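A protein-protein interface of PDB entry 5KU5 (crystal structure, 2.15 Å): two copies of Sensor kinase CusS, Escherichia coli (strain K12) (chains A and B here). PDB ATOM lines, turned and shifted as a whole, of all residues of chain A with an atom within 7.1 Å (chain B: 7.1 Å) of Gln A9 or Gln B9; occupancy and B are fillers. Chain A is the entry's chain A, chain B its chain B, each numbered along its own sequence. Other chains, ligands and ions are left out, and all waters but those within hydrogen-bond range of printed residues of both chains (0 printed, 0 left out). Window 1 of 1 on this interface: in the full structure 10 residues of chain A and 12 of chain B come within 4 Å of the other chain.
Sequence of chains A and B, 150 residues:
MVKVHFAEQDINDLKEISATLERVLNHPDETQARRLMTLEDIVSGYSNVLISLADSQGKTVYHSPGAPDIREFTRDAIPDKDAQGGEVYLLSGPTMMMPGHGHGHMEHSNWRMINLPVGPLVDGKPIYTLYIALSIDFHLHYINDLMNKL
The side-chain amide nitrogen of Gln A9 is in hydrogen-bond range of the side-chain amide oxygen of Gln B9 (3.0 Å).
A ring nitrogen (NE2) of His A139 sits at hydrogen-bond distance from the side-chain carboxylate of Asp A10, 2.7 Å away. O of Glu B8 sits close to OD1 of Asn B12, 3.3 Å away. A ring nitrogen (NE2) of His B139 lies within hydrogen-bond range of the side-chain carboxylate of Asp B10 (2.8 Å).
CG2 of Val A2 touches CG2 of Val B2, 3.7 Å away. NE2 of His A5 touches CZ of Phe B6, at 3.9 Å. CE2 of Phe B138 touches CE1 of His A5, at 3.3 Å. Glu A8 touches Phe B138. Phe B138 touches Gln A9. CE1 of His B139 touches NE2 of Gln A9 (3.5 Å). CE1 of His B5 touches CE2 of Phe A138 (3.3 Å). Glu B8 touches Phe A138 (OE1 to CZ, 3.5 Å). CG of Gln B9 touches CE2 of Phe A138, 3.8 Å away. Gln B9 touches His A139 (NE2 to CE1, 3.6 Å).
Printed residues of chain B within 4 Å of Val A2: Val B2. Of the printed residues of chain B, His A5 touches Phe B6 (3.9 Å) and Phe B138 (3.3 Å). Ala A7 touches none of the printed residues of chain B. Printed residues of chain B within 4 Å of Glu A8: Phe B138. Of the printed residues of chain A, Val B2 touches Val A2. Of the printed residues of chain A, Glu B8 touches Phe A138. Of the printed residues of chain A, Gln B9 touches Gln A9, Phe A138 and His A139. Asp B10 touches none of the printed residues of chain A. The nearest residue of chain B that does not touch Gln A9 is Phe B6 (4.7 Å). The nearest residue of chain A that does not touch Gln B9 is Phe A6 (4.6 Å).
Hydrophobic or aromatic side chains of chain A that line the printed part of chain B: Val A2, His A5, Phe A138 and His A139. Among the printed residues, 11 pairs touch across the chains.
Val B2 touches its own counterpart, Val A2. His A5 touches Phe B138, and with the chains exchanged Phe A138 touches His B5. Glu A8 touches Phe B138, and with the chains exchanged Phe A138 touches Glu B8. Gln B9 touches its own counterpart, Gln A9. Positions printed for both chains: 2, 4, 5, 6, 7, 8, 9, 10, 11, 12, 13, 14, 134, 138 and 139.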
ATOM      1  N   VAL A   2      -4.223   4.481 -10.979  1.00  0.00           N
ATOM      2  CA  VAL A   2      -4.496   3.160 -10.387  1.00  0.00           C
ATOM      3  C   VAL A   2      -3.411   2.692  -9.401  1.00  0.00           C
ATOM      4  O   VAL A   2      -3.722   1.987  -8.437  1.00  0.00           O
ATOM      5  CB  VAL A   2      -4.771   2.080 -11.472  1.00  0.00           C
ATOM      6  CG1 VAL A   2      -3.485   1.587 -12.124  1.00  0.00           C
ATOM      7  CG2 VAL A   2      -5.563   0.921 -10.887  1.00  0.00           C
ATOM      8  N   LYS A   3      -2.162   3.097  -9.640  1.00  0.00           N
ATOM      9  CA  LYS A   3      -1.042   2.770  -8.750  1.00  0.00           C
ATOM     10  C   LYS A   3      -1.218   3.451  -7.391  1.00  0.00           C
ATOM     11  O   LYS A   3      -1.021   2.833  -6.342  1.00  0.00           O
ATOM     12  CB  LYS A   3       0.300   3.189  -9.366  1.00  0.00           C
ATOM     13  CG  LYS A   3       0.825   2.279 -10.468  1.00  0.00           C
ATOM     14  CD  LYS A   3       0.256   2.632 -11.833  1.00  0.00           C
ATOM     15  CE  LYS A   3       0.334   4.127 -12.106  1.00  0.00           C
ATOM     16  NZ  LYS A   3      -0.522   4.530 -13.255  1.00  0.00           N
ATOM     17  N   VAL A   4      -1.586   4.731  -7.426  1.00  0.00           N
ATOM     18  CA  VAL A   4      -1.874   5.506  -6.210  1.00  0.00           C
ATOM     19  C   VAL A   4      -3.071   4.895  -5.474  1.00  0.00           C
ATOM     20  O   VAL A   4      -3.084   4.826  -4.246  1.00  0.00           O
ATOM     21  CB  VAL A   4      -2.135   7.001  -6.537  1.00  0.00           C
ATOM     22  CG1 VAL A   4      -2.705   7.760  -5.339  1.00  0.00           C
ATOM     23  CG2 VAL A   4      -0.850   7.665  -7.017  1.00  0.00           C
ATOM     24  N   HIS A   5      -4.063   4.449  -6.239  1.00  0.00           N
ATOM     25  CA  HIS A   5      -5.230   3.780  -5.684  1.00  0.00           C
ATOM     26  C   HIS A   5      -4.878   2.443  -5.005  1.00  0.00           C
ATOM     27  O   HIS A   5      -5.371   2.153  -3.912  1.00  0.00           O
ATOM     28  CB  HIS A   5      -6.281   3.570  -6.772  1.00  0.00           C
ATOM     29  CG  HIS A   5      -7.522   2.920  -6.266  1.00  0.00           C
ATOM     30  ND1 HIS A   5      -8.510   3.618  -5.611  1.00  0.00           N
ATOM     31  CD2 HIS A   5      -7.912   1.627  -6.275  1.00  0.00           C
ATOM     32  CE1 HIS A   5      -9.466   2.786  -5.249  1.00  0.00           C
ATOM     33  NE2 HIS A   5      -9.128   1.574  -5.645  1.00  0.00           N
ATOM     34  N   PHE A   6      -4.032   1.643  -5.652  1.00  0.00           N
ATOM     35  CA  PHE A   6      -3.516   0.408  -5.045  1.00  0.00           C
ATOM     36  C   PHE A   6      -2.758   0.686  -3.744  1.00  0.00           C
ATOM     37  O   PHE A   6      -2.889  -0.069  -2.780  1.00  0.00           O
ATOM     38  CB  PHE A   6      -2.584  -0.351  -6.007  1.00  0.00           C
ATOM     39  CG  PHE A   6      -3.260  -0.947  -7.229  1.00  0.00           C
ATOM     40  CD1 PHE A   6      -4.646  -1.156  -7.305  1.00  0.00           C
ATOM     41  CD2 PHE A   6      -2.473  -1.362  -8.304  1.00  0.00           C
ATOM     42  CE1 PHE A   6      -5.216  -1.723  -8.440  1.00  0.00           C
ATOM     43  CE2 PHE A   6      -3.044  -1.930  -9.434  1.00  0.00           C
ATOM     44  CZ  PHE A   6      -4.415  -2.113  -9.502  1.00  0.00           C
ATOM     45  N   ALA A   7      -1.971   1.763  -3.722  1.00  0.00           N
ATOM     46  CA  ALA A   7      -1.247   2.164  -2.511  1.00  0.00           C
ATOM     47  C   ALA A   7      -2.205   2.504  -1.378  1.00  0.00           C
ATOM     48  O   ALA A   7      -2.000   2.066  -0.245  1.00  0.00           O
ATOM     49  CB  ALA A   7      -0.320   3.342  -2.791  1.00  0.00           C
ATOM     50  N   GLU A   8      -3.250   3.271  -1.693  1.00  0.00           N
ATOM     51  CA  GLU A   8      -4.250   3.672  -0.692  1.00  0.00           C
ATOM     52  C   GLU A   8      -5.057   2.484  -0.153  1.00  0.00           C
ATOM     53  O   GLU A   8      -5.349   2.437   1.047  1.00  0.00           O
ATOM     54  CB  GLU A   8      -5.188   4.753  -1.251  1.00  0.00           C
ATOM     55  CG  GLU A   8      -4.529   6.116  -1.452  1.00  0.00           C
ATOM     56  CD  GLU A   8      -4.128   6.801  -0.150  1.00  0.00           C
ATOM     57  OE1 GLU A   8      -4.883   6.725   0.845  1.00  0.00           O
ATOM     58  OE2 GLU A   8      -3.048   7.428  -0.119  1.00  0.00           O
ATOM     59  N   GLN A   9      -5.407   1.536  -1.028  1.00  0.00           N
ATOM     60  CA  GLN A   9      -5.988   0.251  -0.597  1.00  0.00           C
ATOM     61  C   GLN A   9      -5.112  -0.419   0.466  1.00  0.00           C
ATOM     62  O   GLN A   9      -5.601  -0.805   1.527  1.00  0.00           O
ATOM     63  CB  GLN A   9      -6.155  -0.724  -1.775  1.00  0.00           C
ATOM     64  CG  GLN A   9      -7.348  -0.476  -2.681  1.00  0.00           C
ATOM     65  CD  GLN A   9      -7.485  -1.560  -3.743  1.00  0.00           C
ATOM     66  OE1 GLN A   9      -6.521  -1.876  -4.447  1.00  0.00           O
ATOM     67  NE2 GLN A   9      -8.678  -2.142  -3.861  1.00  0.00           N
ATOM     68  N   ASP A  10      -3.820  -0.533   0.166  1.00  0.00           N
ATOM     69  CA  ASP A  10      -2.845  -1.160   1.069  1.00  0.00           C
ATOM     70  C   ASP A  10      -2.658  -0.381   2.364  1.00  0.00           C
ATOM     71  O   ASP A  10      -2.652  -0.969   3.443  1.00  0.00           O
ATOM     72  CB  ASP A  10      -1.486  -1.320   0.374  1.00  0.00           C
ATOM     73  CG  ASP A  10      -1.542  -2.264  -0.810  1.00  0.00           C
ATOM     74  OD1 ASP A  10      -2.600  -2.894  -1.026  1.00  0.00           O
ATOM     75  OD2 ASP A  10      -0.534  -2.381  -1.535  1.00  0.00           O
ATOM     76  N   ILE A  11      -2.506   0.937   2.248  1.00  0.00           N
ATOM     77  CA  ILE A  11      -2.351   1.818   3.417  1.00  0.00           C
ATOM     78  C   ILE A  11      -3.528   1.669   4.394  1.00  0.00           C
ATOM     79  O   ILE A  11      -3.322   1.621   5.608  1.00  0.00           O
ATOM     80  CB  ILE A  11      -2.144   3.289   2.980  1.00  0.00           C
ATOM     81  CG1 ILE A  11      -0.727   3.455   2.410  1.00  0.00           C
ATOM     82  CG2 ILE A  11      -2.354   4.263   4.139  1.00  0.00           C
ATOM     83  CD1 ILE A  11      -0.541   4.674   1.532  1.00  0.00           C
ATOM     84  N   ASN A  12      -4.742   1.575   3.855  1.00  0.00           N
ATOM     85  CA  ASN A  12      -5.939   1.347   4.664  1.00  0.00           C
ATOM     86  C   ASN A  12      -5.912   0.004   5.407  1.00  0.00           C
ATOM     87  O   ASN A  12      -6.245  -0.057   6.593  1.00  0.00           O
ATOM     88  CB  ASN A  12      -7.193   1.449   3.788  1.00  0.00           C
ATOM     89  CG  ASN A  12      -8.479   1.288   4.580  1.00  0.00           C
ATOM     90  OD1 ASN A  12      -9.296   0.417   4.282  1.00  0.00           O
ATOM     91  ND2 ASN A  12      -8.658   2.123   5.600  1.00  0.00           N
ATOM     92  N   ASP A  13      -5.523  -1.063   4.708  1.00  0.00           N
ATOM     93  CA  ASP A  13      -5.338  -2.383   5.335  1.00  0.00           C
ATOM     94  C   ASP A  13      -4.255  -2.338   6.417  1.00  0.00           C
ATOM     95  O   ASP A  13      -4.447  -2.873   7.510  1.00  0.00           O
ATOM     96  CB  ASP A  13      -4.979  -3.455   4.294  1.00  0.00           C
ATOM     97  CG  ASP A  13      -6.127  -3.770   3.334  1.00  0.00           C
ATOM     98  OD1 ASP A  13      -7.259  -3.278   3.543  1.00  0.00           O
ATOM     99  OD2 ASP A  13      -5.894  -4.525   2.363  1.00  0.00           O
ATOM    100  N   LEU A  14      -3.129  -1.697   6.111  1.00  0.00           N
ATOM    101  CA  LEU A  14      -2.041  -1.539   7.085  1.00  0.00           C
ATOM    102  C   LEU A  14      -2.452  -0.712   8.309  1.00  0.00           C
ATOM    103  O   LEU A  14      -2.018  -1.006   9.420  1.00  0.00           O
ATOM    104  CB  LEU A  14      -0.801  -0.928   6.429  1.00  0.00           C
ATOM    105  CG  LEU A  14      -0.074  -1.829   5.425  1.00  0.00           C
ATOM    106  CD1 LEU A  14       0.899  -1.010   4.591  1.00  0.00           C
ATOM    107  CD2 LEU A  14       0.647  -2.980   6.120  1.00  0.00           C
ATOM    108  N   LYS A  15      -3.292   0.305   8.106  1.00  0.00           N
ATOM    109  CA  LYS A  15      -3.813   1.099   9.223  1.00  0.00           C
ATOM    110  C   LYS A  15      -4.602   0.225  10.205  1.00  0.00           C
ATOM    111  O   LYS A  15      -4.384   0.299  11.414  1.00  0.00           O
ATOM    112  CB  LYS A  15      -4.688   2.251   8.716  1.00  0.00           C
ATOM    113  CG  LYS A  15      -5.129   3.216   9.809  1.00  0.00           C
ATOM    114  CD  LYS A  15      -6.027   4.312   9.267  1.00  0.00           C
ATOM    115  CE  LYS A  15      -6.566   5.163  10.401  1.00  0.00           C
ATOM    116  NZ  LYS A  15      -7.435   6.259   9.898  1.00  0.00           N
ATOM    117  N   LEU A 134       2.658  -6.036   4.067  1.00  0.00           N
ATOM    118  CA  LEU A 134       1.472  -6.524   3.347  1.00  0.00           C
ATOM    119  C   LEU A 134       1.851  -6.895   1.915  1.00  0.00           C
ATOM    120  O   LEU A 134       2.553  -6.140   1.243  1.00  0.00           O
ATOM    121  CB  LEU A 134       0.379  -5.447   3.322  1.00  0.00           C
ATOM    122  CG  LEU A 134      -0.903  -5.739   2.526  1.00  0.00           C
ATOM    123  CD1 LEU A 134      -1.671  -6.888   3.156  1.00  0.00           C
ATOM    124  CD2 LEU A 134      -1.782  -4.502   2.436  1.00  0.00           C
ATOM    125  N   PHE A 138      -0.258  -9.299  -6.106  1.00  0.00           N
ATOM    126  CA  PHE A 138      -1.443  -9.206  -6.960  1.00  0.00           C
ATOM    127  C   PHE A 138      -1.534  -7.847  -7.668  1.00  0.00           C
ATOM    128  O   PHE A 138      -1.959  -7.797  -8.820  1.00  0.00           O
ATOM    129  CB  PHE A 138      -2.725  -9.514  -6.168  1.00  0.00           C
ATOM    130  CG  PHE A 138      -3.899  -9.899  -7.028  1.00  0.00           C
ATOM    131  CD1 PHE A 138      -3.806 -10.958  -7.935  1.00  0.00           C
ATOM    132  CD2 PHE A 138      -5.113  -9.223  -6.923  1.00  0.00           C
ATOM    133  CE1 PHE A 138      -4.888 -11.317  -8.727  1.00  0.00           C
ATOM    134  CE2 PHE A 138      -6.198  -9.582  -7.708  1.00  0.00           C
ATOM    135  CZ  PHE A 138      -6.087 -10.628  -8.612  1.00  0.00           C
ATOM    136  N   HIS A 139      -1.113  -6.765  -7.002  1.00  0.00           N
ATOM    137  CA  HIS A 139      -0.994  -5.438  -7.650  1.00  0.00           C
ATOM    138  C   HIS A 139      -0.019  -5.480  -8.826  1.00  0.00           C
ATOM    139  O   HIS A 139      -0.336  -5.010  -9.919  1.00  0.00           O
ATOM    140  CB  HIS A 139      -0.516  -4.339  -6.678  1.00  0.00           C
ATOM    141  CG  HIS A 139      -1.443  -4.075  -5.533  1.00  0.00           C
ATOM    142  ND1 HIS A 139      -2.742  -3.669  -5.712  1.00  0.00           N
ATOM    143  CD2 HIS A 139      -1.248  -4.123  -4.194  1.00  0.00           C
ATOM    144  CE1 HIS A 139      -3.318  -3.491  -4.537  1.00  0.00           C
ATOM    145  NE2 HIS A 139      -2.432  -3.763  -3.599  1.00  0.00           N
ATOM    146  N   VAL B   2      -9.780  -2.642 -15.237  1.00  0.00           N
ATOM    147  CA  VAL B   2      -9.621  -2.503 -13.754  1.00  0.00           C
ATOM    148  C   VAL B   2     -10.828  -3.036 -12.957  1.00  0.00           C
ATOM    149  O   VAL B   2     -10.666  -3.482 -11.820  1.00  0.00           O
ATOM    150  CB  VAL B   2      -9.283  -1.038 -13.364  1.00  0.00           C
ATOM    151  CG1 VAL B   2     -10.531  -0.159 -13.283  1.00  0.00           C
ATOM    152  CG2 VAL B   2      -8.503  -0.997 -12.058  1.00  0.00           C
ATOM    153  N   VAL B   4     -12.560  -5.785 -13.576  1.00  0.00           N
ATOM    154  CA  VAL B   4     -12.387  -7.232 -13.410  1.00  0.00           C
ATOM    155  C   VAL B   4     -11.350  -7.501 -12.319  1.00  0.00           C
ATOM    156  O   VAL B   4     -11.517  -8.421 -11.511  1.00  0.00           O
ATOM    157  CB  VAL B   4     -11.969  -7.933 -14.727  1.00  0.00           C
ATOM    158  CG1 VAL B   4     -11.730  -9.425 -14.497  1.00  0.00           C
ATOM    159  CG2 VAL B   4     -13.032  -7.724 -15.801  1.00  0.00           C
ATOM    160  N   HIS B   5     -10.294  -6.691 -12.293  1.00  0.00           N
ATOM    161  CA  HIS B   5      -9.291  -6.790 -11.246  1.00  0.00           C
ATOM    162  C   HIS B   5      -9.875  -6.553  -9.850  1.00  0.00           C
ATOM    163  O   HIS B   5      -9.560  -7.303  -8.917  1.00  0.00           O
ATOM    164  CB  HIS B   5      -8.127  -5.832 -11.477  1.00  0.00           C
ATOM    165  CG  HIS B   5      -7.043  -6.007 -10.470  1.00  0.00           C
ATOM    166  ND1 HIS B   5      -6.088  -6.994 -10.577  1.00  0.00           N
ATOM    167  CD2 HIS B   5      -6.824  -5.394  -9.285  1.00  0.00           C
ATOM    168  CE1 HIS B   5      -5.300  -6.953  -9.519  1.00  0.00           C
ATOM    169  NE2 HIS B   5      -5.724  -5.991  -8.723  1.00  0.00           N
ATOM    170  N   PHE B   6     -10.712  -5.522  -9.715  1.00  0.00           N
ATOM    171  CA  PHE B   6     -11.382  -5.222  -8.439  1.00  0.00           C
ATOM    172  C   PHE B   6     -12.274  -6.372  -7.977  1.00  0.00           C
ATOM    173  O   PHE B   6     -12.308  -6.695  -6.785  1.00  0.00           O
ATOM    174  CB  PHE B   6     -12.229  -3.939  -8.530  1.00  0.00           C
ATOM    175  CG  PHE B   6     -11.437  -2.653  -8.691  1.00  0.00           C
ATOM    176  CD1 PHE B   6     -10.079  -2.550  -8.350  1.00  0.00           C
ATOM    177  CD2 PHE B   6     -12.092  -1.504  -9.130  1.00  0.00           C
ATOM    178  CE1 PHE B   6      -9.399  -1.346  -8.498  1.00  0.00           C
ATOM    179  CE2 PHE B   6     -11.416  -0.302  -9.274  1.00  0.00           C
ATOM    180  CZ  PHE B   6     -10.068  -0.220  -8.953  1.00  0.00           C
ATOM    181  N   ALA B   7     -12.998  -6.973  -8.922  1.00  0.00           N
ATOM    182  CA  ALA B   7     -13.810  -8.163  -8.645  1.00  0.00           C
ATOM    183  C   ALA B   7     -12.955  -9.326  -8.142  1.00  0.00           C
ATOM    184  O   ALA B   7     -13.317  -9.978  -7.163  1.00  0.00           O
ATOM    185  CB  ALA B   7     -14.595  -8.579  -9.882  1.00  0.00           C
ATOM    186  N   GLU B   8     -11.822  -9.570  -8.801  1.00  0.00           N
ATOM    187  CA  GLU B   8     -10.903 -10.641  -8.393  1.00  0.00           C
ATOM    188  C   GLU B   8     -10.305 -10.406  -6.996  1.00  0.00           C
ATOM    189  O   GLU B   8     -10.174 -11.357  -6.224  1.00  0.00           O
ATOM    190  CB  GLU B   8      -9.785 -10.847  -9.424  1.00  0.00           C
ATOM    191  CG  GLU B   8     -10.239 -11.510 -10.720  1.00  0.00           C
ATOM    192  CD  GLU B   8      -9.139 -11.608 -11.771  1.00  0.00           C
ATOM    193  OE1 GLU B   8      -7.945 -11.513 -11.421  1.00  0.00           O
ATOM    194  OE2 GLU B   8      -9.466 -11.790 -12.964  1.00  0.00           O
ATOM    195  N   GLN B   9      -9.949  -9.156  -6.680  1.00  0.00           N
ATOM    196  CA  GLN B   9      -9.493  -8.787  -5.325  1.00  0.00           C
ATOM    197  C   GLN B   9     -10.516  -9.190  -4.262  1.00  0.00           C
ATOM    198  O   GLN B   9     -10.166  -9.810  -3.254  1.00  0.00           O
ATOM    199  CB  GLN B   9      -9.234  -7.276  -5.206  1.00  0.00           C
ATOM    200  CG  GLN B   9      -7.947  -6.782  -5.848  1.00  0.00           C
ATOM    201  CD  GLN B   9      -7.723  -5.287  -5.631  1.00  0.00           C
ATOM    202  OE1 GLN B   9      -8.642  -4.483  -5.787  1.00  0.00           O
ATOM    203  NE2 GLN B   9      -6.496  -4.907  -5.278  1.00  0.00           N
ATOM    204  N   ASP B  10     -11.776  -8.834  -4.512  1.00  0.00           N
ATOM    205  CA  ASP B  10     -12.872  -9.092  -3.577  1.00  0.00           C
ATOM    206  C   ASP B  10     -13.194 -10.579  -3.460  1.00  0.00           C
ATOM    207  O   ASP B  10     -13.426 -11.081  -2.355  1.00  0.00           O
ATOM    208  CB  ASP B  10     -14.135  -8.328  -3.999  1.00  0.00           C
ATOM    209  CG  ASP B  10     -13.955  -6.814  -3.963  1.00  0.00           C
ATOM    210  OD1 ASP B  10     -12.906  -6.331  -3.485  1.00  0.00           O
ATOM    211  OD2 ASP B  10     -14.868  -6.098  -4.427  1.00  0.00           O
ATOM    212  N   ILE B  11     -13.211 -11.276  -4.595  1.00  0.00           N
ATOM    213  CA  ILE B  11     -13.474 -12.719  -4.619  1.00  0.00           C
ATOM    214  C   ILE B  11     -12.418 -13.469  -3.801  1.00  0.00           C
ATOM    215  O   ILE B  11     -12.759 -14.364  -3.029  1.00  0.00           O
ATOM    216  CB  ILE B  11     -13.569 -13.265  -6.070  1.00  0.00           C
ATOM    217  CG1 ILE B  11     -14.841 -12.736  -6.751  1.00  0.00           C
ATOM    218  CG2 ILE B  11     -13.596 -14.792  -6.092  1.00  0.00           C
ATOM    219  CD1 ILE B  11     -14.805 -12.789  -8.267  1.00  0.00           C
ATOM    220  N   ASN B  12     -11.151 -13.086  -3.953  1.00  0.00           N
ATOM    221  CA  ASN B  12     -10.074 -13.658  -3.139  1.00  0.00           C
ATOM    222  C   ASN B  12     -10.323 -13.447  -1.649  1.00  0.00           C
ATOM    223  O   ASN B  12     -10.232 -14.395  -0.867  1.00  0.00           O
ATOM    224  CB  ASN B  12      -8.713 -13.068  -3.523  1.00  0.00           C
ATOM    225  CG  ASN B  12      -8.283 -13.438  -4.935  1.00  0.00           C
ATOM    226  OD1 ASN B  12      -8.880 -14.303  -5.580  1.00  0.00           O
ATOM    227  ND2 ASN B  12      -7.245 -12.770  -5.426  1.00  0.00           N
ATOM    228  N   ASP B  13     -10.653 -12.209  -1.274  1.00  0.00           N
ATOM    229  CA  ASP B  13     -10.981 -11.871   0.118  1.00  0.00           C
ATOM    230  C   ASP B  13     -12.156 -12.690   0.640  1.00  0.00           C
ATOM    231  O   ASP B  13     -12.054 -13.301   1.706  1.00  0.00           O
ATOM    232  CB  ASP B  13     -11.297 -10.374   0.272  1.00  0.00           C
ATOM    233  CG  ASP B  13     -10.061  -9.494   0.209  1.00  0.00           C
ATOM    234  OD1 ASP B  13      -8.930 -10.017   0.077  1.00  0.00           O
ATOM    235  OD2 ASP B  13     -10.227  -8.257   0.298  1.00  0.00           O
ATOM    236  N   LEU B  14     -13.253 -12.709  -0.123  1.00  0.00           N
ATOM    237  CA  LEU B  14     -14.466 -13.457   0.253  1.00  0.00           C
ATOM    238  C   LEU B  14     -14.247 -14.964   0.363  1.00  0.00           C
ATOM    239  O   LEU B  14     -14.800 -15.597   1.261  1.00  0.00           O
ATOM    240  CB  LEU B  14     -15.617 -13.176  -0.724  1.00  0.00           C
ATOM    241  CG  LEU B  14     -16.233 -11.774  -0.651  1.00  0.00           C
ATOM    242  CD1 LEU B  14     -17.112 -11.511  -1.868  1.00  0.00           C
ATOM    243  CD2 LEU B  14     -17.015 -11.576   0.644  1.00  0.00           C
ATOM    244  N   ARG B 112     -20.293  -6.516  -2.294  1.00  0.00           N
ATOM    245  CA  ARG B 112     -20.284  -7.759  -3.056  1.00  0.00           C
ATOM    246  C   ARG B 112     -20.669  -8.876  -2.086  1.00  0.00           C
ATOM    247  O   ARG B 112     -20.100  -8.973  -0.996  1.00  0.00           O
ATOM    248  CB  ARG B 112     -18.924  -8.030  -3.721  1.00  0.00           C
ATOM    249  CG  ARG B 112     -18.964  -7.922  -5.244  1.00  0.00           C
ATOM    250  CD  ARG B 112     -17.646  -8.310  -5.903  1.00  0.00           C
ATOM    251  NE  ARG B 112     -16.767  -7.152  -6.040  1.00  0.00           N
ATOM    252  CZ  ARG B 112     -16.701  -6.326  -7.090  1.00  0.00           C
ATOM    253  NH1 ARG B 112     -17.461  -6.484  -8.174  1.00  0.00           N
ATOM    254  NH2 ARG B 112     -15.845  -5.310  -7.046  1.00  0.00           N
ATOM    255  N   LEU B 134     -19.057  -7.882   1.480  1.00  0.00           N
ATOM    256  CA  LEU B 134     -17.791  -7.148   1.583  1.00  0.00           C
ATOM    257  C   LEU B 134     -17.975  -5.795   0.917  1.00  0.00           C
ATOM    258  O   LEU B 134     -18.499  -5.726  -0.195  1.00  0.00           O
ATOM    259  CB  LEU B 134     -16.665  -7.910   0.867  1.00  0.00           C
ATOM    260  CG  LEU B 134     -15.284  -7.241   0.783  1.00  0.00           C
ATOM    261  CD1 LEU B 134     -14.653  -7.141   2.161  1.00  0.00           C
ATOM    262  CD2 LEU B 134     -14.369  -8.000  -0.164  1.00  0.00           C
ATOM    263  N   PHE B 138     -15.023   1.799  -1.963  1.00  0.00           N
ATOM    264  CA  PHE B 138     -13.736   2.343  -2.417  1.00  0.00           C
ATOM    265  C   PHE B 138     -13.499   2.055  -3.903  1.00  0.00           C
ATOM    266  O   PHE B 138     -12.978   2.915  -4.611  1.00  0.00           O
ATOM    267  CB  PHE B 138     -12.567   1.815  -1.560  1.00  0.00           C
ATOM    268  CG  PHE B 138     -11.303   2.639  -1.658  1.00  0.00           C
ATOM    269  CD1 PHE B 138     -11.326   4.023  -1.470  1.00  0.00           C
ATOM    270  CD2 PHE B 138     -10.077   2.028  -1.907  1.00  0.00           C
ATOM    271  CE1 PHE B 138     -10.164   4.775  -1.555  1.00  0.00           C
ATOM    272  CE2 PHE B 138      -8.911   2.778  -1.988  1.00  0.00           C
ATOM    273  CZ  PHE B 138      -8.955   4.152  -1.815  1.00  0.00           C
ATOM    274  N   HIS B 139     -13.895   0.865  -4.368  1.00  0.00           N
ATOM    275  CA  HIS B 139     -13.870   0.542  -5.808  1.00  0.00           C
ATOM    276  C   HIS B 139     -14.749   1.514  -6.594  1.00  0.00           C
ATOM    277  O   HIS B 139     -14.312   2.078  -7.598  1.00  0.00           O
ATOM    278  CB  HIS B 139     -14.358  -0.891  -6.113  1.00  0.00           C
ATOM    279  CG  HIS B 139     -13.557  -1.979  -5.463  1.00  0.00           C
ATOM    280  ND1 HIS B 139     -12.215  -2.158  -5.703  1.00  0.00           N
ATOM    281  CD2 HIS B 139     -13.919  -2.973  -4.618  1.00  0.00           C
ATOM    282  CE1 HIS B 139     -11.778  -3.201  -5.023  1.00  0.00           C
ATOM    283  NE2 HIS B 139     -12.793  -3.712  -4.352  1.00  0.00           N
